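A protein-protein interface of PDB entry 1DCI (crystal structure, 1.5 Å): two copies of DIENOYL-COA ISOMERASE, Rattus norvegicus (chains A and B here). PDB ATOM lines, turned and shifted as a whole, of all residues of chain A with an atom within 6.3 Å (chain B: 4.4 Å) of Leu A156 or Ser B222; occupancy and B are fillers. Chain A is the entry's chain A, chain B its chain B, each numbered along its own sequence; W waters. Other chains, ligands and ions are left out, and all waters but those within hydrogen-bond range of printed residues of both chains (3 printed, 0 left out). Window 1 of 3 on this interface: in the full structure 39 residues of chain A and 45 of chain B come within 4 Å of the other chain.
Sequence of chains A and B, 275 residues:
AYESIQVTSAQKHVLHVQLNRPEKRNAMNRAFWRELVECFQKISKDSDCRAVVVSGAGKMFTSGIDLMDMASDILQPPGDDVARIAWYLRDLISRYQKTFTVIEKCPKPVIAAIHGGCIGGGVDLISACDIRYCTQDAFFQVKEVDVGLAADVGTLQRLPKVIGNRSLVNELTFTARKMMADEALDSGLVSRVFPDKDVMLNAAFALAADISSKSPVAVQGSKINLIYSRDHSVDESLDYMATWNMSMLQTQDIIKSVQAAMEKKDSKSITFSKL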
ATOM      1  N   ASP A 124      11.811  25.002  16.165  1.00  0.00           N
ATOM      2  CA  ASP A 124      12.705  23.866  16.051  1.00  0.00           C
ATOM      3  C   ASP A 124      11.874  22.602  15.820  1.00  0.00           C
ATOM      4  O   ASP A 124      12.221  21.717  15.047  1.00  0.00           O
ATOM      5  CB  ASP A 124      13.590  23.706  17.284  1.00  0.00           C
ATOM      6  CG  ASP A 124      14.440  24.915  17.649  1.00  0.00           C
ATOM      7  OD1 ASP A 124      13.893  25.824  18.307  1.00  0.00           O
ATOM      8  OD2 ASP A 124      15.653  24.960  17.352  1.00  0.00           O
ATOM      9  N   SER A 127      10.024  22.739  12.226  1.00  0.00           N
ATOM     10  CA  SER A 127      10.935  22.579  11.094  1.00  0.00           C
ATOM     11  C   SER A 127      11.490  21.168  10.980  1.00  0.00           C
ATOM     12  O   SER A 127      12.092  20.879   9.932  1.00  0.00           O
ATOM     13  CB  SER A 127      12.049  23.625  11.120  1.00  0.00           C
ATOM     14  OG  SER A 127      12.800  23.587  12.327  1.00  0.00           O
ATOM     15  N   VAL A 142      11.677  32.911  15.887  1.00  0.00           N
ATOM     16  CA  VAL A 142      12.970  32.286  16.189  1.00  0.00           C
ATOM     17  C   VAL A 142      13.524  33.099  17.357  1.00  0.00           C
ATOM     18  O   VAL A 142      14.312  34.028  17.228  1.00  0.00           O
ATOM     19  CB  VAL A 142      13.935  32.294  15.003  1.00  0.00           C
ATOM     20  CG1 VAL A 142      15.172  31.452  15.295  1.00  0.00           C
ATOM     21  CG2 VAL A 142      13.224  31.731  13.765  1.00  0.00           C
ATOM     22  N   VAL A 145      17.796  34.208  20.025  1.00  0.00           N
ATOM     23  CA  VAL A 145      18.759  35.287  20.249  1.00  0.00           C
ATOM     24  C   VAL A 145      18.299  36.172  21.413  1.00  0.00           C
ATOM     25  O   VAL A 145      19.153  36.691  22.136  1.00  0.00           O
ATOM     26  CB  VAL A 145      19.122  36.165  19.040  1.00  0.00           C
ATOM     27  CG1 VAL A 145      19.837  35.316  17.984  1.00  0.00           C
ATOM     28  CG2 VAL A 145      17.924  36.915  18.507  1.00  0.00           C
ATOM     29  N   LEU A 149      21.244  33.083  23.227  1.00  0.00           N
ATOM     30  CA  LEU A 149      21.922  31.945  22.626  1.00  0.00           C
ATOM     31  C   LEU A 149      21.519  31.771  21.154  1.00  0.00           C
ATOM     32  O   LEU A 149      20.445  32.169  20.774  1.00  0.00           O
ATOM     33  CB  LEU A 149      21.616  30.639  23.376  1.00  0.00           C
ATOM     34  CG  LEU A 149      20.123  30.274  23.495  1.00  0.00           C
ATOM     35  CD1 LEU A 149      19.837  28.995  22.727  1.00  0.00           C
ATOM     36  CD2 LEU A 149      19.773  30.044  24.968  1.00  0.00           C
ATOM     37  N   ALA A 150      22.426  31.138  20.398  1.00  0.00           N
ATOM     38  CA  ALA A 150      22.061  30.739  19.028  1.00  0.00           C
ATOM     39  C   ALA A 150      21.252  29.440  19.166  1.00  0.00           C
ATOM     40  O   ALA A 150      21.683  28.488  19.815  1.00  0.00           O
ATOM     41  CB  ALA A 150      23.347  30.526  18.236  1.00  0.00           C
ATOM     42  N   ALA A 151      20.104  29.391  18.503  1.00  0.00           N
ATOM     43  CA  ALA A 151      19.244  28.210  18.564  1.00  0.00           C
ATOM     44  C   ALA A 151      20.019  26.954  18.258  1.00  0.00           C
ATOM     45  O   ALA A 151      20.668  26.913  17.205  1.00  0.00           O
ATOM     46  CB  ALA A 151      18.104  28.380  17.575  1.00  0.00           C
ATOM     47  N   ASP A 152      19.882  25.911  19.088  1.00  0.00           N
ATOM     48  CA  ASP A 152      20.733  24.745  18.909  1.00  0.00           C
ATOM     49  C   ASP A 152      19.958  23.437  18.800  1.00  0.00           C
ATOM     50  O   ASP A 152      20.601  22.409  18.638  1.00  0.00           O
ATOM     51  CB  ASP A 152      21.793  24.714  20.029  1.00  0.00           C
ATOM     52  CG  ASP A 152      21.236  24.691  21.442  1.00  0.00           C
ATOM     53  OD1 ASP A 152      20.030  24.449  21.610  1.00  0.00           O
ATOM     54  OD2 ASP A 152      21.979  24.944  22.437  1.00  0.00           O
ATOM     55  N   VAL A 153      18.610  23.481  18.824  1.00  0.00           N
ATOM     56  CA  VAL A 153      17.885  22.210  18.747  1.00  0.00           C
ATOM     57  C   VAL A 153      17.208  21.966  17.410  1.00  0.00           C
ATOM     58  O   VAL A 153      16.408  21.028  17.303  1.00  0.00           O
ATOM     59  CB  VAL A 153      16.936  21.979  19.943  1.00  0.00           C
ATOM     60  CG1 VAL A 153      17.778  21.858  21.207  1.00  0.00           C
ATOM     61  CG2 VAL A 153      15.888  23.061  20.056  1.00  0.00           C
ATOM     62  N   GLY A 154      17.663  22.681  16.364  1.00  0.00           N
ATOM     63  CA  GLY A 154      17.231  22.337  15.023  1.00  0.00           C
ATOM     64  C   GLY A 154      16.884  23.441  14.097  1.00  0.00           C
ATOM     65  O   GLY A 154      17.044  23.312  12.867  1.00  0.00           O
ATOM     66  N   THR A 155      16.357  24.560  14.584  1.00  0.00           N
ATOM     67  CA  THR A 155      15.942  25.628  13.676  1.00  0.00           C
ATOM     68  C   THR A 155      17.029  26.053  12.695  1.00  0.00           C
ATOM     69  O   THR A 155      16.776  26.178  11.486  1.00  0.00           O
ATOM     70  CB  THR A 155      15.503  26.868  14.472  1.00  0.00           C
ATOM     71  OG1 THR A 155      14.297  26.482  15.152  1.00  0.00           O
ATOM     72  CG2 THR A 155      15.258  28.075  13.584  1.00  0.00           C
ATOM     73  N   LEU A 156      18.260  26.296  13.182  1.00  0.00           N
ATOM     74  CA  LEU A 156      19.253  26.817  12.242  1.00  0.00           C
ATOM     75  C   LEU A 156      19.617  25.766  11.199  1.00  0.00           C
ATOM     76  O   LEU A 156      20.100  26.108  10.120  1.00  0.00           O
ATOM     77  CB  LEU A 156      20.532  27.268  12.973  1.00  0.00           C
ATOM     78  CG  LEU A 156      20.291  28.284  14.114  1.00  0.00           C
ATOM     79  CD1 LEU A 156      21.642  28.715  14.677  1.00  0.00           C
ATOM     80  CD2 LEU A 156      19.497  29.503  13.664  1.00  0.00           C
ATOM     81  N   GLN A 157      19.497  24.479  11.544  1.00  0.00           N
ATOM     82  CA  GLN A 157      19.911  23.392  10.654  1.00  0.00           C
ATOM     83  C   GLN A 157      18.788  23.043   9.680  1.00  0.00           C
ATOM     84  O   GLN A 157      19.123  22.657   8.542  1.00  0.00           O
ATOM     85  CB  GLN A 157      20.285  22.161  11.483  1.00  0.00           C
ATOM     86  CG  GLN A 157      21.577  22.272  12.288  1.00  0.00           C
ATOM     87  CD  GLN A 157      21.447  23.178  13.505  1.00  0.00           C
ATOM     88  OE1 GLN A 157      20.402  23.172  14.145  1.00  0.00           O
ATOM     89  NE2 GLN A 157      22.503  23.949  13.770  1.00  0.00           N
ATOM     90  N   ARG A 158      17.529  23.197  10.094  1.00  0.00           N
ATOM     91  CA  ARG A 158      16.416  22.802   9.231  1.00  0.00           C
ATOM     92  C   ARG A 158      15.569  23.911   8.654  1.00  0.00           C
ATOM     93  O   ARG A 158      15.072  23.776   7.517  1.00  0.00           O
ATOM     94  CB  ARG A 158      15.491  21.829   9.989  1.00  0.00           C
ATOM     95  CG  ARG A 158      16.125  20.535  10.428  1.00  0.00           C
ATOM     96  CD  ARG A 158      15.073  19.488  10.847  1.00  0.00           C
ATOM     97  NE  ARG A 158      15.750  18.278  11.337  1.00  0.00           N
ATOM     98  CZ  ARG A 158      16.172  18.050  12.583  1.00  0.00           C
ATOM     99  NH1 ARG A 158      15.966  18.975  13.528  1.00  0.00           N
ATOM    100  NH2 ARG A 158      16.821  16.933  12.875  1.00  0.00           N
ATOM    101  N   LEU A 159      15.359  25.035   9.336  1.00  0.00           N
ATOM    102  CA  LEU A 159      14.542  26.111   8.796  1.00  0.00           C
ATOM    103  C   LEU A 159      14.995  26.629   7.441  1.00  0.00           C
ATOM    104  O   LEU A 159      14.179  26.692   6.493  1.00  0.00           O
ATOM    105  CB  LEU A 159      14.347  27.261   9.798  1.00  0.00           C
ATOM    106  CG  LEU A 159      13.579  28.478   9.268  1.00  0.00           C
ATOM    107  CD1 LEU A 159      12.145  28.148   8.911  1.00  0.00           C
ATOM    108  CD2 LEU A 159      13.658  29.604  10.298  1.00  0.00           C
ATOM    109  N   PRO A 160      16.286  26.841   7.204  1.00  0.00           N
ATOM    110  CA  PRO A 160      16.775  27.279   5.903  1.00  0.00           C
ATOM    111  C   PRO A 160      16.658  26.188   4.845  1.00  0.00           C
ATOM    112  O   PRO A 160      16.855  26.474   3.657  1.00  0.00           O
ATOM    113  CB  PRO A 160      18.231  27.681   6.108  1.00  0.00           C
ATOM    114  CG  PRO A 160      18.404  27.757   7.585  1.00  0.00           C
ATOM    115  CD  PRO A 160      17.398  26.808   8.188  1.00  0.00           C
ATOM    116  N   LYS A 161      16.340  24.959   5.268  1.00  0.00           N
ATOM    117  CA  LYS A 161      16.147  23.855   4.346  1.00  0.00           C
ATOM    118  C   LYS A 161      14.677  23.498   4.203  1.00  0.00           C
ATOM    119  O   LYS A 161      14.394  22.398   3.679  1.00  0.00           O
ATOM    120  CB  LYS A 161      16.989  22.647   4.728  1.00  0.00           C
ATOM    121  CG  LYS A 161      18.480  22.916   4.557  1.00  0.00           C
ATOM    122  CD  LYS A 161      19.312  21.767   5.130  1.00  0.00           C
ATOM    123  CE  LYS A 161      20.760  22.094   4.755  1.00  0.00           C
ATOM    124  NZ  LYS A 161      21.699  21.018   5.140  1.00  0.00           N
ATOM    125  N   THR A 173      16.043  35.213  12.254  1.00  0.00           N
ATOM    126  CA  THR A 173      16.979  34.690  13.240  1.00  0.00           C
ATOM    127  C   THR A 173      17.704  35.780  14.011  1.00  0.00           C
ATOM    128  O   THR A 173      17.857  35.673  15.243  1.00  0.00           O
ATOM    129  CB  THR A 173      18.002  33.743  12.577  1.00  0.00           C
ATOM    130  OG1 THR A 173      17.279  32.707  11.890  1.00  0.00           O
ATOM    131  CG2 THR A 173      18.890  33.051  13.610  1.00  0.00           C
ATOM    132  N   PHE A 174      18.216  36.800  13.318  1.00  0.00           N
ATOM    133  CA  PHE A 174      19.023  37.809  14.011  1.00  0.00           C
ATOM    134  C   PHE A 174      18.174  38.797  14.797  1.00  0.00           C
ATOM    135  O   PHE A 174      18.727  39.375  15.764  1.00  0.00           O
ATOM    136  CB  PHE A 174      19.918  38.543  13.008  1.00  0.00           C
ATOM    137  CG  PHE A 174      20.814  37.639  12.207  1.00  0.00           C
ATOM    138  CD1 PHE A 174      21.423  36.504  12.692  1.00  0.00           C
ATOM    139  CD2 PHE A 174      21.078  38.046  10.903  1.00  0.00           C
ATOM    140  CE1 PHE A 174      22.262  35.736  11.901  1.00  0.00           C
ATOM    141  CE2 PHE A 174      21.916  37.283  10.100  1.00  0.00           C
ATOM    142  CZ  PHE A 174      22.515  36.155  10.591  1.00  0.00           C
ATOM    143  N   ALA B 218      25.082  35.342  20.638  1.00  0.00           N
ATOM    144  CA  ALA B 218      23.936  34.666  20.035  1.00  0.00           C
ATOM    145  C   ALA B 218      23.809  34.986  18.542  1.00  0.00           C
ATOM    146  O   ALA B 218      23.642  34.082  17.726  1.00  0.00           O
ATOM    147  CB  ALA B 218      22.649  35.123  20.726  1.00  0.00           C
ATOM    148  N   VAL B 219      23.895  36.273  18.201  1.00  0.00           N
ATOM    149  CA  VAL B 219      23.727  36.667  16.792  1.00  0.00           C
ATOM    150  C   VAL B 219      24.841  36.108  15.919  1.00  0.00           C
ATOM    151  O   VAL B 219      24.560  35.508  14.868  1.00  0.00           O
ATOM    152  CB  VAL B 219      23.661  38.196  16.663  1.00  0.00           C
ATOM    153  CG1 VAL B 219      23.749  38.638  15.201  1.00  0.00           C
ATOM    154  CG2 VAL B 219      22.359  38.764  17.215  1.00  0.00           C
ATOM    155  N   GLN B 220      26.089  36.313  16.320  1.00  0.00           N
ATOM    156  CA  GLN B 220      27.214  35.865  15.462  1.00  0.00           C
ATOM    157  C   GLN B 220      27.355  34.374  15.455  1.00  0.00           C
ATOM    158  O   GLN B 220      27.600  33.765  14.394  1.00  0.00           O
ATOM    159  CB  GLN B 220      28.488  36.587  15.929  1.00  0.00           C
ATOM    160  CG  GLN B 220      28.339  38.097  15.727  1.00  0.00           C
ATOM    161  CD  GLN B 220      29.545  38.865  16.231  1.00  0.00           C
ATOM    162  OE1 GLN B 220      30.684  38.426  16.146  1.00  0.00           O
ATOM    163  NE2 GLN B 220      29.202  40.056  16.762  1.00  0.00           N
ATOM    164  N   GLY B 221      27.111  33.675  16.562  1.00  0.00           N
ATOM    165  CA  GLY B 221      27.036  32.211  16.546  1.00  0.00           C
ATOM    166  C   GLY B 221      25.888  31.760  15.644  1.00  0.00           C
ATOM    167  O   GLY B 221      26.046  30.695  15.029  1.00  0.00           O
ATOM    168  N   SER B 222      24.778  32.475  15.552  1.00  0.00           N
ATOM    169  CA  SER B 222      23.660  32.090  14.679  1.00  0.00           C
ATOM    170  C   SER B 222      24.150  32.218  13.215  1.00  0.00           C
ATOM    171  O   SER B 222      23.876  31.305  12.432  1.00  0.00           O
ATOM    172  CB  SER B 222      22.431  32.972  14.882  1.00  0.00           C
ATOM    173  OG  SER B 222      21.830  32.717  16.174  1.00  0.00           O
ATOM    174  N   LYS B 223      24.794  33.337  12.867  1.00  0.00           N
ATOM    175  CA  LYS B 223      25.283  33.443  11.463  1.00  0.00           C
ATOM    176  C   LYS B 223      26.261  32.326  11.158  1.00  0.00           C
ATOM    177  O   LYS B 223      26.165  31.629  10.117  1.00  0.00           O
ATOM    178  CB  LYS B 223      25.961  34.799  11.224  1.00  0.00           C
ATOM    179  CG  LYS B 223      26.669  34.808   9.841  1.00  0.00           C
ATOM    180  CD  LYS B 223      27.014  36.236   9.402  1.00  0.00           C
ATOM    181  CE  LYS B 223      27.779  36.200   8.056  1.00  0.00           C
ATOM    182  NZ  LYS B 223      28.126  37.605   7.623  1.00  0.00           N
ATOM    183  N   ILE B 224      27.270  32.062  11.981  1.00  0.00           N
ATOM    184  CA  ILE B 224      28.251  31.022  11.750  1.00  0.00           C
ATOM    185  C   ILE B 224      27.565  29.665  11.553  1.00  0.00           C
ATOM    186  O   ILE B 224      27.955  28.948  10.631  1.00  0.00           O
ATOM    187  CB  ILE B 224      29.267  30.963  12.917  1.00  0.00           C
ATOM    188  CG1 ILE B 224      30.164  32.210  12.828  1.00  0.00           C
ATOM    189  CG2 ILE B 224      30.087  29.680  12.964  1.00  0.00           C
ATOM    190  CD1 ILE B 224      30.958  32.487  14.106  1.00  0.00           C
ATOM    191  N   ASN B 225      26.580  29.358  12.403  1.00  0.00           N
ATOM    192  CA  ASN B 225      25.931  28.044  12.256  1.00  0.00           C
ATOM    193  C   ASN B 225      24.927  27.974  11.138  1.00  0.00           C
ATOM    194  O   ASN B 225      24.751  26.871  10.590  1.00  0.00           O
ATOM    195  CB  ASN B 225      25.320  27.618  13.613  1.00  0.00           C
ATOM    196  CG  ASN B 225      26.451  27.086  14.463  1.00  0.00           C
ATOM    197  OD1 ASN B 225      26.934  25.950  14.336  1.00  0.00           O
ATOM    198  ND2 ASN B 225      26.914  27.964  15.389  1.00  0.00           N
ATOM    199  N   LEU B 226      24.298  29.076  10.743  1.00  0.00           N
ATOM    200  CA  LEU B 226      23.416  29.046   9.564  1.00  0.00           C
ATOM    201  C   LEU B 226      24.305  28.754   8.349  1.00  0.00           C
ATOM    202  O   LEU B 226      23.896  27.971   7.469  1.00  0.00           O
ATOM    203  CB  LEU B 226      22.723  30.385   9.387  1.00  0.00           C
ATOM    204  CG  LEU B 226      21.485  30.623  10.270  1.00  0.00           C
ATOM    205  CD1 LEU B 226      21.157  32.108  10.302  1.00  0.00           C
ATOM    206  CD2 LEU B 226      20.287  29.798   9.813  1.00  0.00           C
ATOM    207  N   SER B 229      25.411  25.087   8.451  1.00  0.00           N
ATOM    208  CA  SER B 229      24.263  24.230   8.185  1.00  0.00           C
ATOM    209  C   SER B 229      23.866  24.216   6.721  1.00  0.00           C
ATOM    210  O   SER B 229      23.318  23.226   6.225  1.00  0.00           O
ATOM    211  CB  SER B 229      23.051  24.675   9.033  1.00  0.00           C
ATOM    212  OG  SER B 229      23.339  24.420  10.399  1.00  0.00           O
HETATM  213  O   HOH W   1      19.237  31.651  16.860  1.00  0.00           O
HETATM  214  O   HOH W   2      25.340  24.180  12.758  1.00  0.00           O
HETATM  215  O   HOH W   3      21.752  21.475   7.934  1.00  0.00           O
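O of Ser B229 is in hydrogen-bond range of NZ of Lys A161 (2.9 Å).
The side-chain hydroxyl (OG) of Ser B222 is in hydrogen-bond range of the backbone carbonyl oxygen (O) of Ala B218. O of Gly B221 sits at hydrogen-bond distance from ND2 of Asn B225, at 2.9 Å. OG of Ser B229 lies within hydrogen-bond range of O of Asn B225, at 2.8 Å.
Among the printed residues, pairs that only touch across the chains: Val A145 with Ala B218 (3.9 Å), Val A145 with Ser B222 (3.7 Å), Leu A149 with Ala B218 (3.5 Å), Ala A150 with Ala B218 (3.6 Å), Ala A150 with Gly B221 (3.8 Å), Ala A150 with Ser B222 (3.4 Å), Leu A156 with Ser B222 (3.9 Å), Leu A156 with Asn B225 (3.98 Å), Leu A156 with Leu B226 (3.7 Å), Leu A156 with Ser B229 (3.5 Å), Gln A157 with Ser B229 (3.4 Å), Pro A160 with Leu B226 (3.6 Å), Thr A173 with Ser B222 (3.8 Å), Phe A174 with Val B219 (3.8 Å) and Phe A174 with Lys B223 (3.6 Å).
Of the printed residues of chain B, Leu A156 touches Ser B222 (3.9 Å), Asn B225 (3.98 Å), Leu B226 (3.7 Å) and Ser B229 (3.5 Å). Of the printed residues of chain A, Ser B222 touches Val A145, Ala A150, Leu A156 and Thr A173. Of the printed residues of chain B, Ala A150 touches Ala B218 (3.6 Å), Gly B221 (3.8 Å) and Ser B222 (3.4 Å). Of the printed residues of chain A, Gly B221 touches Ala A150. Of the printed residues of chain B, Val A145 touches Ala B218 and Ser B222. Printed residues of chain B within 4 Å of Thr A173: Ser B222 (3.8 Å). Printed residues of chain B within 4 Å of Lys A161: Ser B229 (2.9 Å). Gly A154 touches none of the printed residues of chain B. The nearest printed residue of chain B that does not touch Lys A161 is Leu B226 (7.2 Å).
Of the 19 printed residues of chain A, 9 touch a printed residue of chain B. Hydrophobic or aromatic side chains of chain A that line the printed part of chain B: Val A145, Ala A150, Leu A156, Pro A160 and Phe A174. Printed residues of chain B that touch a printed residue of chain A: Ala B218, Val B219, Gly B221, Ser B222, Lys B223, Asn B225, Leu B226 and Ser B229. Among the printed residues, 16 pairs touch across the chains.
No position is printed for both chains. Of the 16 pairs that touch across the chains among the printed residues, none has its exchanged pair printed and touching as well.
Water W3 lies within hydrogen-bond range of the side-chain amino group of Lys A161, the backbone carbonyl oxygen of Ser B229 and the backbone carbonyl oxygen of Gln A157. Water W2 lies within hydrogen-bond range of the side-chain amide oxygen of Asn B225 (2.9 Å), the side-chain amide nitrogen of Gln A157 (3.0 Å) and the side-chain hydroxyl of Ser B229 (3.1 Å). Water W1 bridges the side-chain hydroxyl of Ser B222 (2.9 Å) and the backbone NH of Ala A151 (2.9 Å).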
